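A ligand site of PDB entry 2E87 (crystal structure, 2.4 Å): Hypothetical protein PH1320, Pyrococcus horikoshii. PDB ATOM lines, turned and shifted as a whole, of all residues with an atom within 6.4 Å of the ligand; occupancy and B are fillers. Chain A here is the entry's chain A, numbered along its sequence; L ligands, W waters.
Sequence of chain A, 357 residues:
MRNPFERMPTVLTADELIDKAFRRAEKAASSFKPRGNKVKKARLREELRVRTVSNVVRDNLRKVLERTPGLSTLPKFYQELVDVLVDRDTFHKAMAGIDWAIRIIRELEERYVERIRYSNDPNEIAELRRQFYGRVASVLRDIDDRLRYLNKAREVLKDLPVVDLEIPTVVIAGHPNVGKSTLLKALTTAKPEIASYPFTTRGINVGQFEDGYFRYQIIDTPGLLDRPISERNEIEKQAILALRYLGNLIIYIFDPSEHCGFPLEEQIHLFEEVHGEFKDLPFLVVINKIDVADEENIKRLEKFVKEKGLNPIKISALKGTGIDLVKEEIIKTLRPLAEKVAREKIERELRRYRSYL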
ATOM      1  N   GLY A 174      32.080 -17.344  21.394  1.00  0.00           N
ATOM      2  CA  GLY A 174      32.445 -15.969  21.156  1.00  0.00           C
ATOM      3  C   GLY A 174      33.264 -15.443  22.307  1.00  0.00           C
ATOM      4  O   GLY A 174      33.254 -16.025  23.398  1.00  0.00           O
ATOM      5  N   HIS A 175      33.976 -14.335  22.086  1.00  0.00           N
ATOM      6  CA  HIS A 175      34.808 -13.711  23.105  1.00  0.00           C
ATOM      7  C   HIS A 175      34.028 -13.336  24.351  1.00  0.00           C
ATOM      8  O   HIS A 175      32.786 -13.340  24.378  1.00  0.00           O
ATOM      9  CB  HIS A 175      35.479 -12.445  22.558  1.00  0.00           C
ATOM     10  CG  HIS A 175      36.756 -12.688  21.844  1.00  0.00           C
ATOM     11  ND1 HIS A 175      36.855 -12.715  20.464  1.00  0.00           N
ATOM     12  CD2 HIS A 175      38.012 -12.941  22.309  1.00  0.00           C
ATOM     13  CE1 HIS A 175      38.098 -12.956  20.114  1.00  0.00           C
ATOM     14  NE2 HIS A 175      38.821 -13.104  21.213  1.00  0.00           N
ATOM     15  N   PRO A 176      34.741 -12.967  25.412  1.00  0.00           N
ATOM     16  CA  PRO A 176      34.065 -12.580  26.640  1.00  0.00           C
ATOM     17  C   PRO A 176      33.326 -11.278  26.402  1.00  0.00           C
ATOM     18  O   PRO A 176      33.778 -10.439  25.627  1.00  0.00           O
ATOM     19  CB  PRO A 176      35.207 -12.417  27.635  1.00  0.00           C
ATOM     20  CG  PRO A 176      36.288 -13.333  27.070  1.00  0.00           C
ATOM     21  CD  PRO A 176      36.205 -13.024  25.612  1.00  0.00           C
ATOM     22  N   ASN A 177      32.176 -11.141  27.055  1.00  0.00           N
ATOM     23  CA  ASN A 177      31.356  -9.948  26.964  1.00  0.00           C
ATOM     24  C   ASN A 177      30.685  -9.687  25.629  1.00  0.00           C
ATOM     25  O   ASN A 177      30.271  -8.563  25.372  1.00  0.00           O
ATOM     26  CB  ASN A 177      32.157  -8.694  27.328  1.00  0.00           C
ATOM     27  CG  ASN A 177      32.991  -8.865  28.573  1.00  0.00           C
ATOM     28  OD1 ASN A 177      32.481  -9.206  29.635  1.00  0.00           O
ATOM     29  ND2 ASN A 177      34.290  -8.617  28.454  1.00  0.00           N
ATOM     30  N   VAL A 178      30.578 -10.690  24.752  1.00  0.00           N
ATOM     31  CA  VAL A 178      29.914 -10.418  23.486  1.00  0.00           C
ATOM     32  C   VAL A 178      28.403 -10.626  23.572  1.00  0.00           C
ATOM     33  O   VAL A 178      27.677 -10.289  22.654  1.00  0.00           O
ATOM     34  CB  VAL A 178      30.462 -11.282  22.329  1.00  0.00           C
ATOM     35  CG1 VAL A 178      31.931 -11.000  22.111  1.00  0.00           C
ATOM     36  CG2 VAL A 178      30.221 -12.761  22.620  1.00  0.00           C
ATOM     37  N   GLY A 179      27.933 -11.183  24.687  1.00  0.00           N
ATOM     38  CA  GLY A 179      26.512 -11.410  24.865  1.00  0.00           C
ATOM     39  C   GLY A 179      26.044 -12.853  24.895  1.00  0.00           C
ATOM     40  O   GLY A 179      24.851 -13.130  24.752  1.00  0.00           O
ATOM     41  N   LYS A 180      26.974 -13.785  25.070  1.00  0.00           N
ATOM     42  CA  LYS A 180      26.641 -15.195  25.105  1.00  0.00           C
ATOM     43  C   LYS A 180      25.533 -15.532  26.121  1.00  0.00           C
ATOM     44  O   LYS A 180      24.508 -16.088  25.746  1.00  0.00           O
ATOM     45  CB  LYS A 180      27.890 -16.028  25.392  1.00  0.00           C
ATOM     46  CG  LYS A 180      28.937 -15.956  24.279  1.00  0.00           C
ATOM     47  CD  LYS A 180      30.005 -17.048  24.432  1.00  0.00           C
ATOM     48  CE  LYS A 180      30.824 -16.877  25.721  1.00  0.00           C
ATOM     49  NZ  LYS A 180      31.608 -15.598  25.705  1.00  0.00           N
ATOM     50  N   SER A 181      25.749 -15.201  27.391  1.00  0.00           N
ATOM     51  CA  SER A 181      24.749 -15.510  28.418  1.00  0.00           C
ATOM     52  C   SER A 181      23.479 -14.690  28.249  1.00  0.00           C
ATOM     53  O   SER A 181      22.385 -15.161  28.561  1.00  0.00           O
ATOM     54  CB  SER A 181      25.334 -15.287  29.809  1.00  0.00           C
ATOM     55  OG  SER A 181      25.715 -13.941  29.976  1.00  0.00           O
ATOM     56  N   THR A 182      23.614 -13.458  27.772  1.00  0.00           N
ATOM     57  CA  THR A 182      22.462 -12.611  27.564  1.00  0.00           C
ATOM     58  C   THR A 182      21.579 -13.292  26.538  1.00  0.00           C
ATOM     59  O   THR A 182      20.364 -13.327  26.688  1.00  0.00           O
ATOM     60  CB  THR A 182      22.856 -11.192  27.035  1.00  0.00           C
ATOM     61  OG1 THR A 182      23.615 -10.512  28.030  1.00  0.00           O
ATOM     62  CG2 THR A 182      21.600 -10.351  26.720  1.00  0.00           C
ATOM     63  N   LEU A 183      22.205 -13.857  25.514  1.00  0.00           N
ATOM     64  CA  LEU A 183      21.461 -14.562  24.468  1.00  0.00           C
ATOM     65  C   LEU A 183      20.861 -15.865  24.981  1.00  0.00           C
ATOM     66  O   LEU A 183      19.731 -16.219  24.639  1.00  0.00           O
ATOM     67  CB  LEU A 183      22.355 -14.856  23.262  1.00  0.00           C
ATOM     68  CG  LEU A 183      21.702 -15.754  22.222  1.00  0.00           C
ATOM     69  CD1 LEU A 183      20.452 -15.078  21.660  1.00  0.00           C
ATOM     70  CD2 LEU A 183      22.669 -16.024  21.100  1.00  0.00           C
ATOM     71  N   ASN A 205      26.427 -21.823  31.829  1.00  0.00           N
ATOM     72  CA  ASN A 205      24.995 -21.713  31.906  1.00  0.00           C
ATOM     73  C   ASN A 205      24.353 -22.762  31.034  1.00  0.00           C
ATOM     74  O   ASN A 205      24.827 -23.032  29.937  1.00  0.00           O
ATOM     75  CB  ASN A 205      24.553 -20.327  31.452  1.00  0.00           C
ATOM     76  CG  ASN A 205      25.134 -19.241  32.310  1.00  0.00           C
ATOM     77  OD1 ASN A 205      24.766 -19.090  33.464  1.00  0.00           O
ATOM     78  ND2 ASN A 205      26.060 -18.490  31.744  1.00  0.00           N
ATOM     79  N   ASP A 220      26.279 -21.952  27.126  1.00  0.00           N
ATOM     80  CA  ASP A 220      27.273 -20.977  26.660  1.00  0.00           C
ATOM     81  C   ASP A 220      28.645 -21.539  27.035  1.00  0.00           C
ATOM     82  O   ASP A 220      28.739 -22.511  27.794  1.00  0.00           O
ATOM     83  CB  ASP A 220      27.048 -19.574  27.229  1.00  0.00           C
ATOM     84  CG  ASP A 220      27.034 -19.532  28.737  1.00  0.00           C
ATOM     85  OD1 ASP A 220      27.155 -20.583  29.401  1.00  0.00           O
ATOM     86  OD2 ASP A 220      26.908 -18.407  29.256  1.00  0.00           O
ATOM     87  N   PRO A 222      31.704 -19.840  28.400  1.00  0.00           N
ATOM     88  CA  PRO A 222      32.743 -18.978  28.983  1.00  0.00           C
ATOM     89  C   PRO A 222      33.926 -19.825  29.457  1.00  0.00           C
ATOM     90  O   PRO A 222      33.740 -20.893  30.049  1.00  0.00           O
ATOM     91  CB  PRO A 222      32.014 -18.295  30.150  1.00  0.00           C
ATOM     92  CG  PRO A 222      31.078 -19.398  30.619  1.00  0.00           C
ATOM     93  CD  PRO A 222      30.545 -19.976  29.300  1.00  0.00           C
ATOM     94  N   ILE A 253      28.694 -15.671  18.229  1.00  0.00           N
ATOM     95  CA  ILE A 253      28.341 -14.270  18.335  1.00  0.00           C
ATOM     96  C   ILE A 253      29.530 -13.325  18.156  1.00  0.00           C
ATOM     97  O   ILE A 253      30.558 -13.485  18.816  1.00  0.00           O
ATOM     98  CB  ILE A 253      27.721 -13.940  19.704  1.00  0.00           C
ATOM     99  CG1 ILE A 253      26.526 -14.850  20.004  1.00  0.00           C
ATOM    100  CG2 ILE A 253      27.302 -12.482  19.719  1.00  0.00           C
ATOM    101  CD1 ILE A 253      25.889 -14.605  21.369  1.00  0.00           C
ATOM    102  N   HIS A 259      32.671  -3.229  21.996  1.00  0.00           N
ATOM    103  CA  HIS A 259      32.527  -2.833  23.403  1.00  0.00           C
ATOM    104  C   HIS A 259      32.895  -3.999  24.298  1.00  0.00           C
ATOM    105  O   HIS A 259      33.208  -3.810  25.473  1.00  0.00           O
ATOM    106  CB  HIS A 259      31.102  -2.361  23.698  1.00  0.00           C
ATOM    107  CG  HIS A 259      30.727  -1.105  22.965  1.00  0.00           C
ATOM    108  ND1 HIS A 259      29.430  -0.648  22.880  1.00  0.00           N
ATOM    109  CD2 HIS A 259      31.482  -0.224  22.263  1.00  0.00           C
ATOM    110  CE1 HIS A 259      29.398   0.455  22.161  1.00  0.00           C
ATOM    111  NE2 HIS A 259      30.631   0.731  21.773  1.00  0.00           N
ATOM    112  N   ASN A 288      25.665  -9.453  17.116  1.00  0.00           N
ATOM    113  CA  ASN A 288      25.010  -8.815  18.259  1.00  0.00           C
ATOM    114  C   ASN A 288      25.316  -7.340  18.439  1.00  0.00           C
ATOM    115  O   ASN A 288      26.084  -6.773  17.670  1.00  0.00           O
ATOM    116  CB  ASN A 288      25.373  -9.578  19.534  1.00  0.00           C
ATOM    117  CG  ASN A 288      24.413  -9.325  20.678  1.00  0.00           C
ATOM    118  OD1 ASN A 288      23.190  -9.253  20.488  1.00  0.00           O
ATOM    119  ND2 ASN A 288      24.945  -9.224  21.884  1.00  0.00           N
ATOM    120  N   LYS A 289      24.718  -6.734  19.457  1.00  0.00           N
ATOM    121  CA  LYS A 289      24.916  -5.309  19.738  1.00  0.00           C
ATOM    122  C   LYS A 289      24.552  -4.396  18.530  1.00  0.00           C
ATOM    123  O   LYS A 289      25.180  -3.360  18.339  1.00  0.00           O
ATOM    124  CB  LYS A 289      26.373  -5.013  20.151  1.00  0.00           C
ATOM    125  CG  LYS A 289      26.698  -5.171  21.621  1.00  0.00           C
ATOM    126  CD  LYS A 289      27.139  -6.580  21.957  1.00  0.00           C
ATOM    127  CE  LYS A 289      27.570  -6.681  23.414  1.00  0.00           C
ATOM    128  NZ  LYS A 289      28.864  -5.977  23.687  1.00  0.00           N
ATOM    129  N   ILE A 290      23.562  -4.770  17.729  1.00  0.00           N
ATOM    130  CA  ILE A 290      23.211  -3.925  16.595  1.00  0.00           C
ATOM    131  C   ILE A 290      22.606  -2.591  17.060  1.00  0.00           C
ATOM    132  O   ILE A 290      22.579  -1.621  16.303  1.00  0.00           O
ATOM    133  CB  ILE A 290      22.200  -4.604  15.652  1.00  0.00           C
ATOM    134  CG1 ILE A 290      20.921  -4.963  16.417  1.00  0.00           C
ATOM    135  CG2 ILE A 290      22.820  -5.813  15.018  1.00  0.00           C
ATOM    136  CD1 ILE A 290      19.872  -5.615  15.555  1.00  0.00           C
ATOM    137  N   ASP A 291      22.127  -2.551  18.298  1.00  0.00           N
ATOM    138  CA  ASP A 291      21.514  -1.343  18.864  1.00  0.00           C
ATOM    139  C   ASP A 291      22.524  -0.260  19.220  1.00  0.00           C
ATOM    140  O   ASP A 291      22.163   0.903  19.443  1.00  0.00           O
ATOM    141  CB  ASP A 291      20.715  -1.711  20.117  1.00  0.00           C
ATOM    142  CG  ASP A 291      21.577  -2.313  21.219  1.00  0.00           C
ATOM    143  OD1 ASP A 291      22.218  -3.350  20.957  1.00  0.00           O
ATOM    144  OD2 ASP A 291      21.628  -1.764  22.335  1.00  0.00           O
ATOM    145  N   VAL A 292      23.807  -0.622  19.280  1.00  0.00           N
ATOM    146  CA  VAL A 292      24.853   0.327  19.632  1.00  0.00           C
ATOM    147  C   VAL A 292      26.045   0.227  18.679  1.00  0.00           C
ATOM    148  O   VAL A 292      27.006   0.976  18.780  1.00  0.00           O
ATOM    149  CB  VAL A 292      25.336   0.085  21.093  1.00  0.00           C
ATOM    150  CG1 VAL A 292      26.334   1.139  21.504  1.00  0.00           C
ATOM    151  CG2 VAL A 292      24.137   0.135  22.046  1.00  0.00           C
ATOM    152  N   ILE A 315      21.152  -9.038  15.427  1.00  0.00           N
ATOM    153  CA  ILE A 315      20.328  -9.036  16.637  1.00  0.00           C
ATOM    154  C   ILE A 315      20.818  -8.108  17.757  1.00  0.00           C
ATOM    155  O   ILE A 315      21.880  -7.487  17.662  1.00  0.00           O
ATOM    156  CB  ILE A 315      20.251 -10.459  17.300  1.00  0.00           C
ATOM    157  CG1 ILE A 315      21.535 -10.744  18.089  1.00  0.00           C
ATOM    158  CG2 ILE A 315      20.052 -11.546  16.253  1.00  0.00           C
ATOM    159  CD1 ILE A 315      21.475 -11.973  18.994  1.00  0.00           C
ATOM    160  N   SER A 316      20.032  -8.048  18.822  1.00  0.00           N
ATOM    161  CA  SER A 316      20.353  -7.284  20.015  1.00  0.00           C
ATOM    162  C   SER A 316      19.834  -8.131  21.166  1.00  0.00           C
ATOM    163  O   SER A 316      18.665  -8.061  21.527  1.00  0.00           O
ATOM    164  CB  SER A 316      19.661  -5.921  20.027  1.00  0.00           C
ATOM    165  OG  SER A 316      19.761  -5.331  21.321  1.00  0.00           O
ATOM    166  N   ALA A 317      20.711  -8.969  21.717  1.00  0.00           N
ATOM    167  CA  ALA A 317      20.331  -9.850  22.813  1.00  0.00           C
ATOM    168  C   ALA A 317      19.712  -9.080  23.979  1.00  0.00           C
ATOM    169  O   ALA A 317      18.798  -9.586  24.634  1.00  0.00           O
ATOM    170  CB  ALA A 317      21.571 -10.627  23.292  1.00  0.00           C
ATOM    171  N   LEU A 318      20.198  -7.875  24.215  1.00  0.00           N
ATOM    172  CA  LEU A 318      19.700  -7.063  25.325  1.00  0.00           C
ATOM    173  C   LEU A 318      18.261  -6.585  25.113  1.00  0.00           C
ATOM    174  O   LEU A 318      17.434  -6.681  26.020  1.00  0.00           O
ATOM    175  CB  LEU A 318      20.602  -5.850  25.559  1.00  0.00           C
ATOM    176  CG  LEU A 318      20.947  -5.508  27.012  1.00  0.00           C
ATOM    177  CD1 LEU A 318      21.699  -4.192  27.045  1.00  0.00           C
ATOM    178  CD2 LEU A 318      19.695  -5.416  27.860  1.00  0.00           C
ATOM    179  N   LYS A 319      17.966  -6.093  23.913  1.00  0.00           N
ATOM    180  CA  LYS A 319      16.633  -5.583  23.641  1.00  0.00           C
ATOM    181  C   LYS A 319      15.657  -6.530  22.954  1.00  0.00           C
ATOM    182  O   LYS A 319      14.522  -6.135  22.664  1.00  0.00           O
ATOM    183  CB  LYS A 319      16.750  -4.284  22.843  1.00  0.00           C
ATOM    184  CG  LYS A 319      17.393  -3.173  23.634  1.00  0.00           C
ATOM    185  CD  LYS A 319      17.352  -1.881  22.848  1.00  0.00           C
ATOM    186  CE  LYS A 319      17.879  -0.731  23.672  1.00  0.00           C
ATOM    187  NZ  LYS A 319      17.959   0.495  22.823  1.00  0.00           N
HETATM  188  P1  LIG L   1      29.212 -13.087  27.632  1.00  0.00           P
HETATM  189  O1  LIG L   1      30.421 -12.800  28.494  1.00  0.00           O
HETATM  190  O2  LIG L   1      29.621 -13.358  26.087  1.00  0.00           O
HETATM  191  O3  LIG L   1      28.093 -13.951  28.235  1.00  0.00           O
HETATM  192  O4  LIG L   1      28.522 -11.656  27.538  1.00  0.00           O
HETATM  193  P2  LIG L   1      27.211 -11.086  28.299  1.00  0.00           P
HETATM  194  O5  LIG L   1      26.005 -11.889  27.957  1.00  0.00           O
HETATM  195  O6  LIG L   1      27.487 -11.117  29.900  1.00  0.00           O
HETATM  196  O7  LIG L   1      27.008  -9.583  27.785  1.00  0.00           O
HETATM  197  C1  LIG L   1      28.167  -8.813  28.155  1.00  0.00           C
HETATM  198  C2  LIG L   1      27.779  -7.334  28.324  1.00  0.00           C
HETATM  199  O8  LIG L   1      27.168  -6.831  27.067  1.00  0.00           O
HETATM  200  C3  LIG L   1      26.706  -7.059  29.376  1.00  0.00           C
HETATM  201  O9  LIG L   1      26.698  -6.042  30.369  1.00  0.00           O
HETATM  202  C4  LIG L   1      25.395  -7.257  28.580  1.00  0.00           C
HETATM  203  O10 LIG L   1      24.378  -6.473  29.234  1.00  0.00           O
HETATM  204  C5  LIG L   1      25.763  -6.450  27.350  1.00  0.00           C
HETATM  205  N1  LIG L   1      24.939  -6.785  26.179  1.00  0.00           N
HETATM  206  C6  LIG L   1      24.478  -8.026  25.807  1.00  0.00           C
HETATM  207  N2  LIG L   1      23.771  -7.930  24.709  1.00  0.00           N
HETATM  208  C7  LIG L   1      23.731  -6.632  24.315  1.00  0.00           C
HETATM  209  C8  LIG L   1      23.118  -5.927  23.221  1.00  0.00           C
HETATM  210  O11 LIG L   1      22.461  -6.522  22.376  1.00  0.00           O
HETATM  211  N3  LIG L   1      23.308  -4.565  23.136  1.00  0.00           N
HETATM  212  C9  LIG L   1      24.058  -3.891  24.092  1.00  0.00           C
HETATM  213  N4  LIG L   1      24.221  -2.536  23.983  1.00  0.00           N
HETATM  214  N5  LIG L   1      24.618  -4.530  25.098  1.00  0.00           N
HETATM  215  C10 LIG L   1      24.480  -5.884  25.254  1.00  0.00           C
HETATM  216  O   HOH W   1      31.964 -14.290  29.800  1.00  0.00           O
HETATM  217  O   HOH W   2      28.964 -16.660  29.094  1.00  0.00           O
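A nitrogen (N3) of the ligand lies within hydrogen-bond range of the side-chain carboxylate (OD1) of Asp 291, at 2.7 Å. O5 of the ligand lies within hydrogen-bond range of N of Thr 182 (2.9 Å). An oxygen (O5) of the ligand sits at hydrogen-bond distance from the side-chain hydroxyl of Thr 182 (2.8 Å). An oxygen (O3) of the ligand lies within hydrogen-bond range of the backbone NH (N) of Ser 181, 2.8 Å away. OG of Ser 181 is in hydrogen-bond range of O5 of the ligand (2.9 Å). N of Asn 177 lies within hydrogen-bond range of O1 of the ligand (2.8 Å). The backbone NH (N) of Lys 180 lies within hydrogen-bond range of an oxygen (O2) of the ligand. An oxygen (O2) of the ligand is in salt-bridge range of the side-chain amino group of Lys 180 (3.0 Å). O4 of the ligand is in hydrogen-bond range of N of Gly 179 (2.9 Å). An oxygen (O11) of the ligand sits at hydrogen-bond distance from the backbone NH of Ala 317 (3.1 Å). The side-chain hydroxyl (OG) of Ser 316 is in hydrogen-bond range of an oxygen (O11) of the ligand (3.1 Å). N of Val 178 sits at hydrogen-bond distance from O2 of the ligand (3.1 Å). An oxygen (O11) of the ligand is in hydrogen-bond range of the backbone NH (N) of Leu 318 (3.2 Å). The side-chain amide nitrogen (ND2) of Asn 288 is in hydrogen-bond range of a nitrogen (N2) of the ligand.
OG of Ser 316 is in hydrogen-bond range of OD1 of Asp 291 (3.2 Å). O of Asn 177 is in hydrogen-bond range of NZ of Lys 289 (3.4 Å). The side-chain amino group (NZ) of Lys 180 sits at hydrogen-bond distance from the backbone carbonyl oxygen (O) of His 175 (2.9 Å). The side-chain amino group (NZ) of Lys 180 is in hydrogen-bond range of the backbone carbonyl oxygen (O) of Gly 174, 2.9 Å away. N of Ala 317 is in hydrogen-bond range of OD1 of Asn 288 (2.8 Å). The side-chain hydroxyl of Ser 316 sits at hydrogen-bond distance from the backbone NH of Lys 319, 3.2 Å away. O of Val 178 lies within hydrogen-bond range of ND2 of Asn 288 (3.0 Å). The backbone NH (N) of Lys 289 lies within hydrogen-bond range of the backbone carbonyl oxygen (O) of Ile 315 (3.4 Å).
O of His 175 touches O2 of the ligand (3.6 Å). C of Pro 176 touches O1 of the ligand, at 3.9 Å. Lys 289 touches the ligand (CE to O8, 3.7 Å). CG2 of Val 292 touches N4 of the ligand, 3.3 Å away. Within 4 Å of the ligand: His 175, Pro 176, Asn 177, Val 178, Gly 179, Lys 180, Ser 181, Thr 182, Asn 288, Lys 289, Asp 291, Val 292, Ser 316, Ala 317 and Leu 318. Along chain A the residues within 4 Å of the ligand span positions 175 to 318.
Water W2 lies within hydrogen-bond range of OD2 of Asp 220 (2.7 Å) and O3 of the ligand (3.0 Å).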
